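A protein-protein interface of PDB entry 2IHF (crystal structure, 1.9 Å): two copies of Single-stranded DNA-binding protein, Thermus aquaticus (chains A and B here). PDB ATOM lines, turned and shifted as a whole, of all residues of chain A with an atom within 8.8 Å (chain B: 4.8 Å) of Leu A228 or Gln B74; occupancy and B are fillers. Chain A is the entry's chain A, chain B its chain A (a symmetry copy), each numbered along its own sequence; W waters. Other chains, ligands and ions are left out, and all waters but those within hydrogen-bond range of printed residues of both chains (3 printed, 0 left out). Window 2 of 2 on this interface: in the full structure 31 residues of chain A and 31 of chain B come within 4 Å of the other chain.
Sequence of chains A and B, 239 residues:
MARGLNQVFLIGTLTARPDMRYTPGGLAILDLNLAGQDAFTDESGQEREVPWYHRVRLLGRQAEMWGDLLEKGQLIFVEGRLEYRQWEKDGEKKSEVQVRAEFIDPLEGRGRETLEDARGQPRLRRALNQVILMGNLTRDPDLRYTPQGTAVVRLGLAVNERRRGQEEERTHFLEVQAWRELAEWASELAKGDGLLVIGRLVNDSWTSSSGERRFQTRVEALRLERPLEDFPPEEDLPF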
ATOM      1  N   ARG A   3      -5.455 -29.982 -18.744  1.00  0.00           N
ATOM      2  CA  ARG A   3      -4.873 -29.283 -19.886  1.00  0.00           C
ATOM      3  C   ARG A   3      -3.768 -30.207 -20.358  1.00  0.00           C
ATOM      4  O   ARG A   3      -3.873 -30.818 -21.408  1.00  0.00           O
ATOM      5  CB  ARG A   3      -4.232 -27.964 -19.480  1.00  0.00           C
ATOM      6  CG  ARG A   3      -3.272 -27.422 -20.527  1.00  0.00           C
ATOM      7  CD  ARG A   3      -3.983 -26.484 -21.474  1.00  0.00           C
ATOM      8  NE  ARG A   3      -4.805 -27.174 -22.458  1.00  0.00           N
ATOM      9  CZ  ARG A   3      -4.311 -27.933 -23.431  1.00  0.00           C
ATOM     10  NH1 ARG A   3      -2.999 -28.097 -23.540  1.00  0.00           N
ATOM     11  NH2 ARG A   3      -5.124 -28.518 -24.305  1.00  0.00           N
ATOM     12  N   MET A 134      -1.869 -34.415 -24.289  1.00  0.00           N
ATOM     13  CA  MET A 134      -2.670 -33.214 -24.458  1.00  0.00           C
ATOM     14  C   MET A 134      -1.735 -32.081 -24.075  1.00  0.00           C
ATOM     15  O   MET A 134      -1.051 -32.145 -23.050  1.00  0.00           O
ATOM     16  CB  MET A 134      -3.925 -33.232 -23.580  1.00  0.00           C
ATOM     17  CG  MET A 134      -4.837 -32.034 -23.808  1.00  0.00           C
ATOM     18  SD  MET A 134      -6.606 -32.351 -23.511  1.00  0.00           S
ATOM     19  CE  MET A 134      -6.568 -33.575 -22.205  1.00  0.00           C
ATOM     20  N   GLY A 194      -4.207 -25.735 -28.620  1.00  0.00           N
ATOM     21  CA  GLY A 194      -4.313 -26.914 -27.780  1.00  0.00           C
ATOM     22  C   GLY A 194      -4.503 -28.141 -28.651  1.00  0.00           C
ATOM     23  O   GLY A 194      -5.097 -28.070 -29.729  1.00  0.00           O
ATOM     24  N   LEU A 195      -3.980 -29.274 -28.203  1.00  0.00           N
ATOM     25  CA  LEU A 195      -4.125 -30.488 -28.975  1.00  0.00           C
ATOM     26  C   LEU A 195      -4.144 -31.750 -28.114  1.00  0.00           C
ATOM     27  O   LEU A 195      -3.408 -31.857 -27.130  1.00  0.00           O
ATOM     28  CB  LEU A 195      -3.004 -30.576 -30.003  1.00  0.00           C
ATOM     29  CG  LEU A 195      -3.100 -31.736 -30.998  1.00  0.00           C
ATOM     30  CD1 LEU A 195      -4.260 -31.502 -31.959  1.00  0.00           C
ATOM     31  CD2 LEU A 195      -1.790 -31.854 -31.755  1.00  0.00           C
ATOM     32  N   LEU A 196      -5.026 -32.678 -28.487  1.00  0.00           N
ATOM     33  CA  LEU A 196      -5.164 -33.981 -27.831  1.00  0.00           C
ATOM     34  C   LEU A 196      -4.631 -34.992 -28.834  1.00  0.00           C
ATOM     35  O   LEU A 196      -5.099 -35.049 -29.971  1.00  0.00           O
ATOM     36  CB  LEU A 196      -6.634 -34.317 -27.529  1.00  0.00           C
ATOM     37  CG  LEU A 196      -6.919 -35.787 -27.163  1.00  0.00           C
ATOM     38  CD1 LEU A 196      -6.146 -36.158 -25.907  1.00  0.00           C
ATOM     39  CD2 LEU A 196      -8.408 -36.009 -26.955  1.00  0.00           C
ATOM     40  N   GLU A 225      -7.373 -34.312 -31.968  1.00  0.00           N
ATOM     41  CA  GLU A 225      -8.590 -33.548 -31.691  1.00  0.00           C
ATOM     42  C   GLU A 225      -8.218 -32.216 -31.066  1.00  0.00           C
ATOM     43  O   GLU A 225      -7.153 -32.090 -30.466  1.00  0.00           O
ATOM     44  CB  GLU A 225      -9.509 -34.289 -30.715  1.00  0.00           C
ATOM     45  CG  GLU A 225     -10.006 -35.667 -31.154  1.00  0.00           C
ATOM     46  CD  GLU A 225     -10.891 -35.629 -32.387  1.00  0.00           C
ATOM     47  OE1 GLU A 225     -11.565 -34.606 -32.622  1.00  0.00           O
ATOM     48  OE2 GLU A 225     -10.921 -36.639 -33.116  1.00  0.00           O
ATOM     49  N   ARG A 226      -9.098 -31.228 -31.191  1.00  0.00           N
ATOM     50  CA  ARG A 226      -8.833 -29.910 -30.626  1.00  0.00           C
ATOM     51  C   ARG A 226      -9.661 -29.648 -29.397  1.00  0.00           C
ATOM     52  O   ARG A 226     -10.886 -29.622 -29.472  1.00  0.00           O
ATOM     53  CB  ARG A 226      -9.139 -28.788 -31.626  1.00  0.00           C
ATOM     54  CG  ARG A 226      -8.244 -28.730 -32.842  1.00  0.00           C
ATOM     55  CD  ARG A 226      -8.372 -27.393 -33.573  1.00  0.00           C
ATOM     56  NE  ARG A 226      -8.052 -26.254 -32.709  1.00  0.00           N
ATOM     57  CZ  ARG A 226      -7.823 -25.018 -33.155  1.00  0.00           C
ATOM     58  NH1 ARG A 226      -7.879 -24.766 -34.454  1.00  0.00           N
ATOM     59  NH2 ARG A 226      -7.536 -24.036 -32.308  1.00  0.00           N
ATOM     60  N   PRO A 227      -9.000 -29.443 -28.241  1.00  0.00           N
ATOM     61  CA  PRO A 227      -9.722 -29.169 -26.997  1.00  0.00           C
ATOM     62  C   PRO A 227     -10.255 -27.750 -27.137  1.00  0.00           C
ATOM     63  O   PRO A 227      -9.480 -26.830 -27.396  1.00  0.00           O
ATOM     64  CB  PRO A 227      -8.631 -29.240 -25.924  1.00  0.00           C
ATOM     65  CG  PRO A 227      -7.528 -30.022 -26.559  1.00  0.00           C
ATOM     66  CD  PRO A 227      -7.556 -29.576 -27.988  1.00  0.00           C
ATOM     67  N   LEU A 228     -11.563 -27.566 -26.984  1.00  0.00           N
ATOM     68  CA  LEU A 228     -12.157 -26.232 -27.098  1.00  0.00           C
ATOM     69  C   LEU A 228     -11.688 -25.290 -25.981  1.00  0.00           C
ATOM     70  O   LEU A 228     -11.408 -25.726 -24.855  1.00  0.00           O
ATOM     71  CB  LEU A 228     -13.689 -26.313 -27.047  1.00  0.00           C
ATOM     72  CG  LEU A 228     -14.474 -26.923 -28.208  1.00  0.00           C
ATOM     73  CD1 LEU A 228     -15.965 -26.834 -27.911  1.00  0.00           C
ATOM     74  CD2 LEU A 228     -14.152 -26.187 -29.494  1.00  0.00           C
ATOM     75  N   GLU A 229     -11.582 -24.000 -26.289  1.00  0.00           N
ATOM     76  CA  GLU A 229     -11.196 -23.059 -25.269  1.00  0.00           C
ATOM     77  C   GLU A 229     -12.220 -21.961 -25.044  1.00  0.00           C
ATOM     78  O   GLU A 229     -12.632 -21.284 -25.980  1.00  0.00           O
ATOM     79  CB  GLU A 229      -9.792 -22.527 -25.528  1.00  0.00           C
ATOM     80  CG  GLU A 229      -8.710 -23.356 -24.853  1.00  0.00           C
ATOM     81  CD  GLU A 229      -7.767 -24.021 -25.832  1.00  0.00           C
ATOM     82  OE1 GLU A 229      -8.054 -23.986 -27.045  1.00  0.00           O
ATOM     83  OE2 GLU A 229      -6.735 -24.576 -25.401  1.00  0.00           O
ATOM     84  N   ASP A 230     -12.628 -21.780 -23.788  1.00  0.00           N
ATOM     85  CA  ASP A 230     -12.496 -20.449 -23.205  1.00  0.00           C
ATOM     86  C   ASP A 230     -13.824 -20.129 -22.525  1.00  0.00           C
ATOM     87  O   ASP A 230     -14.859 -20.696 -22.873  1.00  0.00           O
ATOM     88  CB  ASP A 230     -11.916 -19.470 -24.230  1.00  0.00           C
ATOM     89  CG  ASP A 230     -12.448 -18.061 -24.057  1.00  0.00           C
ATOM     90  OD1 ASP A 230     -12.766 -17.681 -22.910  1.00  0.00           O
ATOM     91  OD2 ASP A 230     -12.583 -17.264 -25.007  1.00  0.00           O
ATOM     92  N   PHE A 231     -13.915 -19.246 -21.641  1.00  0.00           N
ATOM     93  CA  PHE A 231     -14.919 -19.354 -20.572  1.00  0.00           C
ATOM     94  C   PHE A 231     -14.433 -19.166 -19.128  1.00  0.00           C
ATOM     95  O   PHE A 231     -13.376 -19.698 -18.731  1.00  0.00           O
ATOM     96  CB  PHE A 231     -15.591 -20.727 -20.661  1.00  0.00           C
ATOM     97  CG  PHE A 231     -14.752 -21.831 -20.087  1.00  0.00           C
ATOM     98  CD1 PHE A 231     -13.451 -22.041 -20.543  1.00  0.00           C
ATOM     99  CD2 PHE A 231     -15.236 -22.620 -19.051  1.00  0.00           C
ATOM    100  CE1 PHE A 231     -12.650 -23.014 -19.972  1.00  0.00           C
ATOM    101  CE2 PHE A 231     -14.441 -23.598 -18.471  1.00  0.00           C
ATOM    102  CZ  PHE A 231     -13.147 -23.796 -18.929  1.00  0.00           C
ATOM    103  N   GLY B  12     -17.036 -39.250 -27.026  1.00  0.00           N
ATOM    104  CA  GLY B  12     -18.369 -39.471 -27.540  1.00  0.00           C
ATOM    105  C   GLY B  12     -19.088 -38.146 -27.666  1.00  0.00           C
ATOM    106  O   GLY B  12     -18.511 -37.093 -27.375  1.00  0.00           O
ATOM    107  N   THR B  13     -20.348 -38.202 -28.092  1.00  0.00           N
ATOM    108  CA  THR B  13     -21.163 -37.008 -28.276  1.00  0.00           C
ATOM    109  C   THR B  13     -22.313 -36.954 -27.269  1.00  0.00           C
ATOM    110  O   THR B  13     -22.927 -37.973 -26.975  1.00  0.00           O
ATOM    111  CB  THR B  13     -21.753 -36.980 -29.700  1.00  0.00           C
ATOM    112  OG1 THR B  13     -20.694 -37.070 -30.660  1.00  0.00           O
ATOM    113  CG2 THR B  13     -22.520 -35.697 -29.928  1.00  0.00           C
ATOM    114  N   LEU B  14     -22.596 -35.766 -26.737  1.00  0.00           N
ATOM    115  CA  LEU B  14     -23.690 -35.620 -25.785  1.00  0.00           C
ATOM    116  C   LEU B  14     -25.025 -35.810 -26.500  1.00  0.00           C
ATOM    117  O   LEU B  14     -25.277 -35.210 -27.548  1.00  0.00           O
ATOM    118  CB  LEU B  14     -23.662 -34.243 -25.111  1.00  0.00           C
ATOM    119  CG  LEU B  14     -22.523 -33.978 -24.124  1.00  0.00           C
ATOM    120  CD1 LEU B  14     -22.528 -32.519 -23.722  1.00  0.00           C
ATOM    121  CD2 LEU B  14     -22.669 -34.865 -22.897  1.00  0.00           C
ATOM    122  N   LEU B  69     -22.483 -24.817 -19.758  1.00  0.00           N
ATOM    123  CA  LEU B  69     -21.777 -24.539 -21.002  1.00  0.00           C
ATOM    124  C   LEU B  69     -21.960 -25.655 -22.021  1.00  0.00           C
ATOM    125  O   LEU B  69     -22.000 -25.405 -23.223  1.00  0.00           O
ATOM    126  CB  LEU B  69     -20.285 -24.349 -20.753  1.00  0.00           C
ATOM    127  CG  LEU B  69     -19.856 -23.075 -20.035  1.00  0.00           C
ATOM    128  CD1 LEU B  69     -18.335 -23.055 -19.955  1.00  0.00           C
ATOM    129  CD2 LEU B  69     -20.379 -21.847 -20.777  1.00  0.00           C
ATOM    130  N   LEU B  70     -22.080 -26.886 -21.536  1.00  0.00           N
ATOM    131  CA  LEU B  70     -22.219 -28.038 -22.415  1.00  0.00           C
ATOM    132  C   LEU B  70     -23.595 -28.168 -23.054  1.00  0.00           C
ATOM    133  O   LEU B  70     -24.617 -28.083 -22.376  1.00  0.00           O
ATOM    134  CB  LEU B  70     -21.869 -29.317 -21.646  1.00  0.00           C
ATOM    135  CG  LEU B  70     -20.490 -29.345 -20.968  1.00  0.00           C
ATOM    136  CD1 LEU B  70     -20.311 -30.639 -20.193  1.00  0.00           C
ATOM    137  CD2 LEU B  70     -19.395 -29.189 -22.010  1.00  0.00           C
ATOM    138  N   GLU B  71     -23.603 -28.379 -24.367  1.00  0.00           N
ATOM    139  CA  GLU B  71     -24.834 -28.530 -25.135  1.00  0.00           C
ATOM    140  C   GLU B  71     -24.898 -29.883 -25.848  1.00  0.00           C
ATOM    141  O   GLU B  71     -23.875 -30.511 -26.123  1.00  0.00           O
ATOM    142  CB  GLU B  71     -24.941 -27.416 -26.186  1.00  0.00           C
ATOM    143  CG  GLU B  71     -24.943 -25.994 -25.626  1.00  0.00           C
ATOM    144  CD  GLU B  71     -26.309 -25.546 -25.117  1.00  0.00           C
ATOM    145  OE1 GLU B  71     -27.244 -25.431 -25.941  1.00  0.00           O
ATOM    146  OE2 GLU B  71     -26.447 -25.304 -23.895  1.00  0.00           O
ATOM    147  N   LYS B  72     -26.116 -30.323 -26.136  1.00  0.00           N
ATOM    148  CA  LYS B  72     -26.355 -31.568 -26.840  1.00  0.00           C
ATOM    149  C   LYS B  72     -25.607 -31.526 -28.172  1.00  0.00           C
ATOM    150  O   LYS B  72     -25.562 -30.480 -28.821  1.00  0.00           O
ATOM    151  CB  LYS B  72     -27.856 -31.709 -27.090  1.00  0.00           C
ATOM    152  CG  LYS B  72     -28.259 -32.828 -28.017  1.00  0.00           C
ATOM    153  CD  LYS B  72     -29.765 -32.800 -28.233  1.00  0.00           C
ATOM    154  CE  LYS B  72     -30.234 -34.017 -29.001  1.00  0.00           C
ATOM    155  NZ  LYS B  72     -29.546 -34.131 -30.317  1.00  0.00           N
ATOM    156  N   GLY B  73     -25.025 -32.658 -28.577  1.00  0.00           N
ATOM    157  CA  GLY B  73     -24.290 -32.717 -29.834  1.00  0.00           C
ATOM    158  C   GLY B  73     -22.803 -32.413 -29.691  1.00  0.00           C
ATOM    159  O   GLY B  73     -22.032 -32.547 -30.641  1.00  0.00           O
ATOM    160  N   GLN B  74     -22.410 -32.009 -28.487  1.00  0.00           N
ATOM    161  CA  GLN B  74     -21.033 -31.659 -28.148  1.00  0.00           C
ATOM    162  C   GLN B  74     -20.098 -32.882 -28.070  1.00  0.00           C
ATOM    163  O   GLN B  74     -20.423 -33.863 -27.400  1.00  0.00           O
ATOM    164  CB  GLN B  74     -21.029 -30.968 -26.787  1.00  0.00           C
ATOM    165  CG  GLN B  74     -19.827 -30.115 -26.510  1.00  0.00           C
ATOM    166  CD  GLN B  74     -20.099 -28.653 -26.784  1.00  0.00           C
ATOM    167  OE1 GLN B  74     -20.875 -28.008 -26.072  1.00  0.00           O
ATOM    168  NE2 GLN B  74     -19.471 -28.123 -27.823  1.00  0.00           N
ATOM    169  N   LEU B  75     -18.941 -32.822 -28.732  1.00  0.00           N
ATOM    170  CA  LEU B  75     -17.989 -33.931 -28.674  1.00  0.00           C
ATOM    171  C   LEU B  75     -17.149 -33.753 -27.398  1.00  0.00           C
ATOM    172  O   LEU B  75     -16.604 -32.675 -27.145  1.00  0.00           O
ATOM    173  CB  LEU B  75     -17.100 -33.948 -29.922  1.00  0.00           C
ATOM    174  CG  LEU B  75     -16.183 -35.159 -30.146  1.00  0.00           C
ATOM    175  CD1 LEU B  75     -16.981 -36.433 -30.349  1.00  0.00           C
ATOM    176  CD2 LEU B  75     -15.327 -34.886 -31.359  1.00  0.00           C
ATOM    177  N   ILE B  76     -17.058 -34.812 -26.594  1.00  0.00           N
ATOM    178  CA  ILE B  76     -16.331 -34.753 -25.324  1.00  0.00           C
ATOM    179  C   ILE B  76     -15.319 -35.875 -25.123  1.00  0.00           C
ATOM    180  O   ILE B  76     -15.587 -37.020 -25.449  1.00  0.00           O
ATOM    181  CB  ILE B  76     -17.304 -34.843 -24.114  1.00  0.00           C
ATOM    182  CG1 ILE B  76     -18.477 -33.872 -24.274  1.00  0.00           C
ATOM    183  CG2 ILE B  76     -16.543 -34.572 -22.813  1.00  0.00           C
ATOM    184  CD1 ILE B  76     -18.110 -32.426 -24.109  1.00  0.00           C
ATOM    185  N   PRO B 106     -14.117 -30.876 -23.551  1.00  0.00           N
ATOM    186  CA  PRO B 106     -14.930 -30.770 -24.768  1.00  0.00           C
ATOM    187  C   PRO B 106     -13.975 -30.551 -25.939  1.00  0.00           C
ATOM    188  O   PRO B 106     -12.974 -29.842 -25.813  1.00  0.00           O
ATOM    189  CB  PRO B 106     -15.800 -29.544 -24.500  1.00  0.00           C
ATOM    190  CG  PRO B 106     -15.993 -29.601 -23.013  1.00  0.00           C
ATOM    191  CD  PRO B 106     -14.606 -29.952 -22.511  1.00  0.00           C
ATOM    192  N   LEU B 107     -14.288 -31.170 -27.069  1.00  0.00           N
ATOM    193  CA  LEU B 107     -13.461 -31.071 -28.258  1.00  0.00           C
ATOM    194  C   LEU B 107     -14.209 -30.338 -29.359  1.00  0.00           C
ATOM    195  O   LEU B 107     -15.435 -30.369 -29.413  1.00  0.00           O
ATOM    196  CB  LEU B 107     -13.101 -32.485 -28.755  1.00  0.00           C
ATOM    197  CG  LEU B 107     -12.472 -33.444 -27.734  1.00  0.00           C
ATOM    198  CD1 LEU B 107     -12.359 -34.836 -28.321  1.00  0.00           C
ATOM    199  CD2 LEU B 107     -11.114 -32.914 -27.313  1.00  0.00           C
ATOM    200  N   GLU B 108     -13.466 -29.676 -30.234  1.00  0.00           N
ATOM    201  CA  GLU B 108     -14.050 -28.991 -31.377  1.00  0.00           C
ATOM    202  C   GLU B 108     -14.703 -30.109 -32.218  1.00  0.00           C
ATOM    203  O   GLU B 108     -14.035 -31.060 -32.644  1.00  0.00           O
ATOM    204  CB  GLU B 108     -12.919 -28.301 -32.149  1.00  0.00           C
ATOM    205  CG  GLU B 108     -13.280 -27.049 -32.915  1.00  0.00           C
ATOM    206  CD  GLU B 108     -12.087 -26.100 -33.036  1.00  0.00           C
ATOM    207  OE1 GLU B 108     -11.948 -25.195 -32.178  1.00  0.00           O
ATOM    208  OE2 GLU B 108     -11.278 -26.270 -33.976  1.00  0.00           O
HETATM  209  O   HOH W   1     -11.361 -28.582 -23.450  1.00  0.00           O
HETATM  210  O   HOH W   2     -11.527 -31.829 -32.537  1.00  0.00           O
HETATM  211  O   HOH W   3     -11.512 -23.283 -29.650  1.00  0.00           O
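No position is printed for both chains.
Water W2 lies within hydrogen-bond range of O of Glu B108 (2.6 Å), OE1 of Glu A225 (2.8 Å) and N of Arg A226 (2.8 Å). Water W1 lies within hydrogen-bond range of the backbone carbonyl oxygen (O) of Pro B106 (3.1 Å) and the backbone carbonyl oxygen (O) of Leu A228 (3.2 Å). Water W3 lies within hydrogen-bond range of OE1 of Glu B108 (3.2 Å) and N of Glu A229 (3.4 Å).
The side-chain carboxylate (OE2) of Glu B108 is in salt-bridge range of the guanidinium group (NE) of Arg A226 (3.5 Å). O of Pro B106 is in hydrogen-bond range of N of Leu A228.
Of the 14 printed residues of chain B, 6 touch a printed residue of chain A. Hydrophobic or aromatic side chains of chain B that line the printed part of chain A: Leu B69, Leu B75 and Leu B107. Among the printed residues, Asp or Glu carboxylates within 4 Å of a Lys or Arg side-chain nitrogen of the other chain: Arg A226 with Glu B108 (3.5 Å).
Among the printed residues, merely in contact across the chains: Arg A226 with Leu B107 (3.2 Å), Phe A231 with Leu B69 (3.3 Å), Leu A228 with Glu B108 (3.4 Å), Pro A227 with Pro B106 (3.5 Å), Leu A228 with Leu B107 (3.6 Å), Leu A228 with Gln B74 (3.7 Å), Glu A225 with Leu B107 (3.8 Å) and Glu A225 with Leu B75 (3.98 Å).
Arg A3 touches none of the printed residues of chain B. Of the printed residues of chain B, Arg A226 touches Leu B107 (3.2 Å) and Glu B108 (2.7 Å). Leu A228 touches just these residues of chain B: Gln B74, Pro B106, Leu B107 and Glu B108. Leu B70 touches none of the printed residues of chain A. No residue of chain A comes within 4 Å of Gly B73. Of chain A, only Leu A228 comes within 4 Å of Gln B74. Of the printed residues of chain A, Pro B106 touches Pro A227 and Leu A228. Printed residues of chain A within 4 Å of Glu B108: Arg A226 (2.7 Å) and Leu A228 (3.4 Å). The nearest printed residue of chain A that does not touch Gln B74 is Arg A226 (8.9 Å). The nearest printed residue of chain B that does not touch Pro A227 is Leu B107 (4.01 Å).
The backbone NH (N) of Leu B107 sits at hydrogen-bond distance from the backbone carbonyl oxygen (O) of Leu B75 (2.8 Å). N of Leu B14 lies within hydrogen-bond range of O of Gln B74 (3.0 Å). The backbone NH (N) of Leu A196 is in hydrogen-bond range of the backbone carbonyl oxygen (O) of Glu A225, at 3.0 Å. The backbone NH of Glu B71 sits at hydrogen-bond distance from the side-chain amide oxygen of Gln B74, 3.2 Å away.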
